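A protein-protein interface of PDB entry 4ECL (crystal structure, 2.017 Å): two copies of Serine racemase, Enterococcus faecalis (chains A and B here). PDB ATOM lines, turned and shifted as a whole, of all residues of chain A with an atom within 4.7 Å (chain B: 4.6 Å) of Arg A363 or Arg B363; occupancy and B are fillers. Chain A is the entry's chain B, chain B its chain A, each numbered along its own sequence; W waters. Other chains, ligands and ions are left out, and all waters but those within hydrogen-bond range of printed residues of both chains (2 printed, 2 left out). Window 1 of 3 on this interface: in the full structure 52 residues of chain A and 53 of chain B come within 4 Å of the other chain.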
ATOM      1  N   TYR A 284      -1.009 -18.293 -12.266  1.00  0.00           N
ATOM      2  CA  TYR A 284      -1.230 -19.631 -11.718  1.00  0.00           C
ATOM      3  C   TYR A 284      -0.520 -20.737 -12.497  1.00  0.00           C
ATOM      4  O   TYR A 284      -0.179 -21.774 -11.932  1.00  0.00           O
ATOM      5  CB  TYR A 284      -2.718 -19.948 -11.463  1.00  0.00           C
ATOM      6  CG  TYR A 284      -3.652 -19.760 -12.641  1.00  0.00           C
ATOM      7  CD1 TYR A 284      -3.655 -20.653 -13.703  1.00  0.00           C
ATOM      8  CD2 TYR A 284      -4.562 -18.697 -12.674  1.00  0.00           C
ATOM      9  CE1 TYR A 284      -4.528 -20.484 -14.786  1.00  0.00           C
ATOM     10  CE2 TYR A 284      -5.441 -18.532 -13.743  1.00  0.00           C
ATOM     11  CZ  TYR A 284      -5.412 -19.420 -14.794  1.00  0.00           C
ATOM     12  OH  TYR A 284      -6.266 -19.252 -15.853  1.00  0.00           O
ATOM     13  N   ALA A 285      -0.248 -20.498 -13.774  1.00  0.00           N
ATOM     14  CA  ALA A 285       0.488 -21.477 -14.567  1.00  0.00           C
ATOM     15  C   ALA A 285       1.921 -21.662 -14.057  1.00  0.00           C
ATOM     16  O   ALA A 285       2.545 -22.685 -14.321  1.00  0.00           O
ATOM     17  CB  ALA A 285       0.484 -21.101 -16.039  1.00  0.00           C
ATOM     18  N   ASP A 286       2.439 -20.670 -13.339  1.00  0.00           N
ATOM     19  CA  ASP A 286       3.765 -20.779 -12.748  1.00  0.00           C
ATOM     20  C   ASP A 286       3.701 -21.355 -11.334  1.00  0.00           C
ATOM     21  O   ASP A 286       4.718 -21.487 -10.665  1.00  0.00           O
ATOM     22  CB  ASP A 286       4.460 -19.412 -12.729  1.00  0.00           C
ATOM     23  CG  ASP A 286       4.633 -18.833 -14.115  1.00  0.00           C
ATOM     24  OD1 ASP A 286       5.425 -19.404 -14.897  1.00  0.00           O
ATOM     25  OD2 ASP A 286       3.973 -17.813 -14.418  1.00  0.00           O
ATOM     26  N   GLY A 287       2.500 -21.675 -10.868  1.00  0.00           N
ATOM     27  CA  GLY A 287       2.356 -22.287  -9.557  1.00  0.00           C
ATOM     28  C   GLY A 287       2.044 -21.327  -8.432  1.00  0.00           C
ATOM     29  O   GLY A 287       2.063 -21.696  -7.254  1.00  0.00           O
ATOM     30  N   PRO A 289      -0.765 -19.779  -6.652  1.00  0.00           N
ATOM     31  CA  PRO A 289      -2.168 -20.205  -6.661  1.00  0.00           C
ATOM     32  C   PRO A 289      -3.169 -19.104  -7.011  1.00  0.00           C
ATOM     33  O   PRO A 289      -3.051 -17.957  -6.578  1.00  0.00           O
ATOM     34  CB  PRO A 289      -2.382 -20.732  -5.239  1.00  0.00           C
ATOM     35  CG  PRO A 289      -1.013 -21.210  -4.828  1.00  0.00           C
ATOM     36  CD  PRO A 289      -0.081 -20.170  -5.409  1.00  0.00           C
ATOM     37  N   GLU A 359       2.278 -28.722  -0.748  1.00  0.00           N
ATOM     38  CA  GLU A 359       1.623 -28.604  -2.049  1.00  0.00           C
ATOM     39  C   GLU A 359       2.130 -27.352  -2.772  1.00  0.00           C
ATOM     40  O   GLU A 359       2.446 -27.400  -3.969  1.00  0.00           O
ATOM     41  CB  GLU A 359       0.101 -28.570  -1.914  1.00  0.00           C
ATOM     42  CG  GLU A 359      -0.611 -28.509  -3.260  1.00  0.00           C
ATOM     43  CD  GLU A 359      -2.128 -28.480  -3.157  1.00  0.00           C
ATOM     44  OE1 GLU A 359      -2.663 -28.103  -2.090  1.00  0.00           O
ATOM     45  OE2 GLU A 359      -2.788 -28.848  -4.152  1.00  0.00           O
ATOM     46  N   LEU A 360       2.238 -26.248  -2.034  1.00  0.00           N
ATOM     47  CA  LEU A 360       2.618 -24.963  -2.635  1.00  0.00           C
ATOM     48  C   LEU A 360       4.008 -25.033  -3.248  1.00  0.00           C
ATOM     49  O   LEU A 360       4.228 -24.563  -4.369  1.00  0.00           O
ATOM     50  CB  LEU A 360       2.577 -23.834  -1.604  1.00  0.00           C
ATOM     51  CG  LEU A 360       3.118 -22.485  -2.109  1.00  0.00           C
ATOM     52  CD1 LEU A 360       2.176 -21.920  -3.160  1.00  0.00           C
ATOM     53  CD2 LEU A 360       3.301 -21.508  -0.960  1.00  0.00           C
ATOM     54  N   LEU A 361       4.948 -25.617  -2.507  1.00  0.00           N
ATOM     55  CA  LEU A 361       6.323 -25.693  -2.976  1.00  0.00           C
ATOM     56  C   LEU A 361       6.490 -26.707  -4.100  1.00  0.00           C
ATOM     57  O   LEU A 361       7.076 -26.398  -5.136  1.00  0.00           O
ATOM     58  CB  LEU A 361       7.263 -26.031  -1.829  1.00  0.00           C
ATOM     59  CG  LEU A 361       7.402 -24.936  -0.784  1.00  0.00           C
ATOM     60  CD1 LEU A 361       8.413 -25.357   0.290  1.00  0.00           C
ATOM     61  CD2 LEU A 361       7.784 -23.620  -1.454  1.00  0.00           C
ATOM     62  N   SER A 362       5.969 -27.913  -3.901  1.00  0.00           N
ATOM     63  CA  SER A 362       6.120 -28.970  -4.897  1.00  0.00           C
ATOM     64  C   SER A 362       5.390 -28.679  -6.211  1.00  0.00           C
ATOM     65  O   SER A 362       5.668 -29.317  -7.231  1.00  0.00           O
ATOM     66  CB  SER A 362       5.690 -30.340  -4.336  1.00  0.00           C
ATOM     67  OG  SER A 362       4.284 -30.426  -4.177  1.00  0.00           O
ATOM     68  N   ARG A 363       4.469 -27.719  -6.194  1.00  0.00           N
ATOM     69  CA  ARG A 363       3.760 -27.342  -7.414  1.00  0.00           C
ATOM     70  C   ARG A 363       4.242 -26.037  -8.046  1.00  0.00           C
ATOM     71  O   ARG A 363       3.537 -25.432  -8.864  1.00  0.00           O
ATOM     72  CB  ARG A 363       2.254 -27.306  -7.168  1.00  0.00           C
ATOM     73  CG  ARG A 363       1.694 -28.686  -6.788  1.00  0.00           C
ATOM     74  CD  ARG A 363       0.186 -28.666  -6.616  1.00  0.00           C
ATOM     75  NE  ARG A 363      -0.503 -28.386  -7.871  1.00  0.00           N
ATOM     76  CZ  ARG A 363      -1.772 -28.004  -7.953  1.00  0.00           C
ATOM     77  NH1 ARG A 363      -2.506 -27.857  -6.851  1.00  0.00           N
ATOM     78  NH2 ARG A 363      -2.308 -27.769  -9.142  1.00  0.00           N
ATOM     79  N   MET A 364       5.448 -25.611  -7.688  1.00  0.00           N
ATOM     80  CA  MET A 364       6.050 -24.456  -8.351  1.00  0.00           C
ATOM     81  C   MET A 364       6.200 -24.838  -9.811  1.00  0.00           C
ATOM     82  O   MET A 364       6.571 -25.969 -10.122  1.00  0.00           O
ATOM     83  CB  MET A 364       7.404 -24.108  -7.737  1.00  0.00           C
ATOM     84  CG  MET A 364       7.306 -23.421  -6.379  1.00  0.00           C
ATOM     85  SD  MET A 364       6.640 -21.579  -6.570  1.00  0.00           S
ATOM     86  CE  MET A 364       5.096 -21.646  -5.388  1.00  0.00           C
ATOM     87  N   GLY A 365       5.871 -23.916 -10.703  1.00  0.00           N
ATOM     88  CA  GLY A 365       5.815 -24.227 -12.120  1.00  0.00           C
ATOM     89  C   GLY A 365       7.173 -24.540 -12.702  1.00  0.00           C
ATOM     90  O   GLY A 365       8.186 -23.994 -12.285  1.00  0.00           O
ATOM     91  N   TYR B 284      -0.524 -34.704  -5.590  1.00  0.00           N
ATOM     92  CA  TYR B 284      -0.688 -33.286  -5.909  1.00  0.00           C
ATOM     93  C   TYR B 284       0.524 -32.703  -6.639  1.00  0.00           C
ATOM     94  O   TYR B 284       0.376 -31.804  -7.448  1.00  0.00           O
ATOM     95  CB  TYR B 284      -1.132 -32.453  -4.701  1.00  0.00           C
ATOM     96  CG  TYR B 284      -0.270 -32.563  -3.456  1.00  0.00           C
ATOM     97  CD1 TYR B 284       0.981 -31.956  -3.392  1.00  0.00           C
ATOM     98  CD2 TYR B 284      -0.732 -33.228  -2.328  1.00  0.00           C
ATOM     99  CE1 TYR B 284       1.763 -32.040  -2.246  1.00  0.00           C
ATOM    100  CE2 TYR B 284       0.039 -33.315  -1.173  1.00  0.00           C
ATOM    101  CZ  TYR B 284       1.285 -32.721  -1.141  1.00  0.00           C
ATOM    102  OH  TYR B 284       2.048 -32.813  -0.009  1.00  0.00           O
ATOM    103  N   ALA B 285       1.714 -33.253  -6.411  1.00  0.00           N
ATOM    104  CA  ALA B 285       2.885 -32.808  -7.173  1.00  0.00           C
ATOM    105  C   ALA B 285       2.734 -33.089  -8.665  1.00  0.00           C
ATOM    106  O   ALA B 285       3.393 -32.466  -9.492  1.00  0.00           O
ATOM    107  CB  ALA B 285       4.152 -33.438  -6.649  1.00  0.00           C
ATOM    108  N   GLY B 287       0.041 -32.468 -10.089  1.00  0.00           N
ATOM    109  CA  GLY B 287      -0.954 -31.494 -10.499  1.00  0.00           C
ATOM    110  C   GLY B 287      -2.379 -31.942 -10.284  1.00  0.00           C
ATOM    111  O   GLY B 287      -3.313 -31.325 -10.783  1.00  0.00           O
ATOM    112  N   PRO B 289      -5.023 -31.731  -7.810  1.00  0.00           N
ATOM    113  CA  PRO B 289      -5.189 -30.832  -6.655  1.00  0.00           C
ATOM    114  C   PRO B 289      -5.527 -31.533  -5.335  1.00  0.00           C
ATOM    115  O   PRO B 289      -6.456 -32.328  -5.270  1.00  0.00           O
ATOM    116  CB  PRO B 289      -6.365 -29.946  -7.069  1.00  0.00           C
ATOM    117  CG  PRO B 289      -6.393 -30.012  -8.562  1.00  0.00           C
ATOM    118  CD  PRO B 289      -5.923 -31.378  -8.924  1.00  0.00           C
ATOM    119  N   GLU B 359      -6.930 -23.376 -15.031  1.00  0.00           N
ATOM    120  CA  GLU B 359      -5.941 -23.577 -13.971  1.00  0.00           C
ATOM    121  C   GLU B 359      -5.643 -25.063 -13.747  1.00  0.00           C
ATOM    122  O   GLU B 359      -4.484 -25.455 -13.586  1.00  0.00           O
ATOM    123  CB  GLU B 359      -6.391 -22.920 -12.659  1.00  0.00           C
ATOM    124  CG  GLU B 359      -5.428 -23.188 -11.501  1.00  0.00           C
ATOM    125  CD  GLU B 359      -5.951 -22.743 -10.145  1.00  0.00           C
ATOM    126  OE1 GLU B 359      -7.172 -22.508  -9.998  1.00  0.00           O
ATOM    127  OE2 GLU B 359      -5.125 -22.640  -9.214  1.00  0.00           O
ATOM    128  N   LEU B 360      -6.688 -25.887 -13.736  1.00  0.00           N
ATOM    129  CA  LEU B 360      -6.514 -27.329 -13.545  1.00  0.00           C
ATOM    130  C   LEU B 360      -5.580 -27.892 -14.607  1.00  0.00           C
ATOM    131  O   LEU B 360      -4.632 -28.608 -14.299  1.00  0.00           O
ATOM    132  CB  LEU B 360      -7.860 -28.048 -13.620  1.00  0.00           C
ATOM    133  CG  LEU B 360      -7.809 -29.575 -13.454  1.00  0.00           C
ATOM    134  CD1 LEU B 360      -7.402 -29.952 -12.026  1.00  0.00           C
ATOM    135  CD2 LEU B 360      -9.144 -30.223 -13.842  1.00  0.00           C
ATOM    136  N   LEU B 361      -5.826 -27.510 -15.852  1.00  0.00           N
ATOM    137  CA  LEU B 361      -5.107 -28.069 -16.987  1.00  0.00           C
ATOM    138  C   LEU B 361      -3.715 -27.506 -17.157  1.00  0.00           C
ATOM    139  O   LEU B 361      -2.762 -28.260 -17.364  1.00  0.00           O
ATOM    140  CB  LEU B 361      -5.903 -27.875 -18.281  1.00  0.00           C
ATOM    141  CG  LEU B 361      -7.212 -28.661 -18.402  1.00  0.00           C
ATOM    142  CD1 LEU B 361      -7.641 -28.731 -19.857  1.00  0.00           C
ATOM    143  CD2 LEU B 361      -7.102 -30.060 -17.806  1.00  0.00           C
ATOM    144  N   SER B 362      -3.589 -26.180 -17.081  1.00  0.00           N
ATOM    145  CA  SER B 362      -2.287 -25.545 -17.243  1.00  0.00           C
ATOM    146  C   SER B 362      -1.339 -25.940 -16.119  1.00  0.00           C
ATOM    147  O   SER B 362      -0.122 -25.859 -16.280  1.00  0.00           O
ATOM    148  CB  SER B 362      -2.402 -24.016 -17.338  1.00  0.00           C
ATOM    149  OG  SER B 362      -2.752 -23.436 -16.096  1.00  0.00           O
ATOM    150  N   ARG B 363      -1.886 -26.371 -14.985  1.00  0.00           N
ATOM    151  CA  ARG B 363      -1.033 -26.783 -13.858  1.00  0.00           C
ATOM    152  C   ARG B 363      -0.839 -28.294 -13.741  1.00  0.00           C
ATOM    153  O   ARG B 363      -0.516 -28.806 -12.664  1.00  0.00           O
ATOM    154  CB  ARG B 363      -1.553 -26.214 -12.529  1.00  0.00           C
ATOM    155  CG  ARG B 363      -1.598 -24.677 -12.482  1.00  0.00           C
ATOM    156  CD  ARG B 363      -2.076 -24.171 -11.124  1.00  0.00           C
ATOM    157  NE  ARG B 363      -1.207 -24.622 -10.039  1.00  0.00           N
ATOM    158  CZ  ARG B 363      -1.510 -24.523  -8.747  1.00  0.00           C
ATOM    159  NH1 ARG B 363      -2.673 -23.993  -8.371  1.00  0.00           N
ATOM    160  NH2 ARG B 363      -0.648 -24.956  -7.830  1.00  0.00           N
ATOM    161  N   MET B 364      -1.035 -29.017 -14.840  1.00  0.00           N
ATOM    162  CA  MET B 364      -0.713 -30.440 -14.854  1.00  0.00           C
ATOM    163  C   MET B 364       0.786 -30.550 -14.627  1.00  0.00           C
ATOM    164  O   MET B 364       1.562 -29.779 -15.201  1.00  0.00           O
ATOM    165  CB  MET B 364      -1.116 -31.065 -16.185  1.00  0.00           C
ATOM    166  CG  MET B 364      -2.620 -31.320 -16.325  1.00  0.00           C
ATOM    167  SD  MET B 364      -3.222 -32.771 -15.149  1.00  0.00           S
ATOM    168  CE  MET B 364      -4.294 -31.830 -13.834  1.00  0.00           C
ATOM    169  N   GLY B 365       1.195 -31.484 -13.773  1.00  0.00           N
ATOM    170  CA  GLY B 365       2.581 -31.555 -13.338  1.00  0.00           C
ATOM    171  C   GLY B 365       3.522 -31.981 -14.449  1.00  0.00           C
ATOM    172  O   GLY B 365       3.171 -32.796 -15.301  1.00  0.00           O
HETATM  173  O   HOH W   1       1.318 -25.461 -10.421  1.00  0.00           O
HETATM  174  O   HOH W   2       1.932 -24.165  -5.868  1.00  0.00           O
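Printed residues of chain A that touch a printed residue of chain B: Tyr A284, Ala A285, Glu A359, Ser A362 and Arg A363.
Hydrophobic or aromatic side chains of chain A within 4 Å of the printed part of chain B: Tyr A284 and Ala A285.
Of the 11 printed residues of chain B, 6 touch a printed residue of chain A.
Printed residues of chain B that touch a printed residue of chain A: Tyr B284, Ala B285, Pro B289, Glu B359, Ser B362 and Arg B363.
Hydrophobic or aromatic side chains of chain B within 4 Å of the printed part of chain A: Tyr B284 and Ala B285.
Among the printed residues, 10 pairs touch across the chains.
Among the printed residues, no Asp or Glu carboxylate lies within 4 Å of a Lys or Arg side-chain nitrogen of the other chain.
Tyr A284 touches Ser B362, and with the chains exchanged Ser A362 touches Tyr B284.
Tyr A284 touches Arg B363, and with the chains exchanged Arg A363 touches Tyr B284.
Glu A359 touches Pro B289, but with the chains exchanged Pro A289 does not touch Glu B359 (4.6 Å).
Arg B363 touches its own counterpart, Arg A363.
CE1 of Tyr A284 touches CA of Glu B359, 3.5 Å away.
OG of Ser B362 touches CE1 of Tyr A284 (3.7 Å).
Tyr A284 touches Arg B363 (O to CD, 3.2 Å).
Ser B362 touches Ala A285.
CA of Glu A359 touches CE1 of Tyr B284 (3.4 Å).
Glu A359 touches Pro B289.
Tyr B284 touches Ser A362.
CB of Ala B285 touches OG of Ser A362, 3.9 Å away.
CD of Arg A363 touches O of Tyr B284, 3.3 Å away.
Of the printed residues of chain B, Arg A363 touches Tyr B284 (3.3 Å) and Arg B363 (3.3 Å).
Arg B363 touches two residues of chain A.
Printed residues of chain B within 4 Å of Ser A362: Tyr B284 and Ala B285.
Of the printed residues of chain B, Tyr A284 touches Glu B359, Ser B362 and Arg B363.
Of the printed residues of chain A, Glu B359 touches Tyr A284.
Of the printed residues of chain A, Pro B289 touches Glu A359.
The nearest printed residue of chain B that does not touch Arg A363 is Pro B289 (4.01 Å).
Water W1 bridges the guanidinium group (NE) of Arg B363 and the backbone carbonyl oxygen (O) of Arg A363.
Water W2 lies within hydrogen-bond range of the backbone carbonyl oxygen (O) of Leu A360 (2.8 Å), the backbone carbonyl oxygen (O) of Gly A287 (2.8 Å) and the guanidinium group (NH2) of Arg B363 (3.3 Å).
The guanidinium group (NH2) of Arg B363 lies close to the guanidinium group (NE) of Arg A363 (3.4 Å).
The guanidinium group (NH1) of Arg B363 lies within salt-bridge range of the side-chain carboxylate (OE2) of Glu B359, at 2.9 Å.
The side-chain carboxylate (OE2) of Glu A359 lies within salt-bridge range of the guanidinium group (NH1) of Arg A363, 2.9 Å away.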
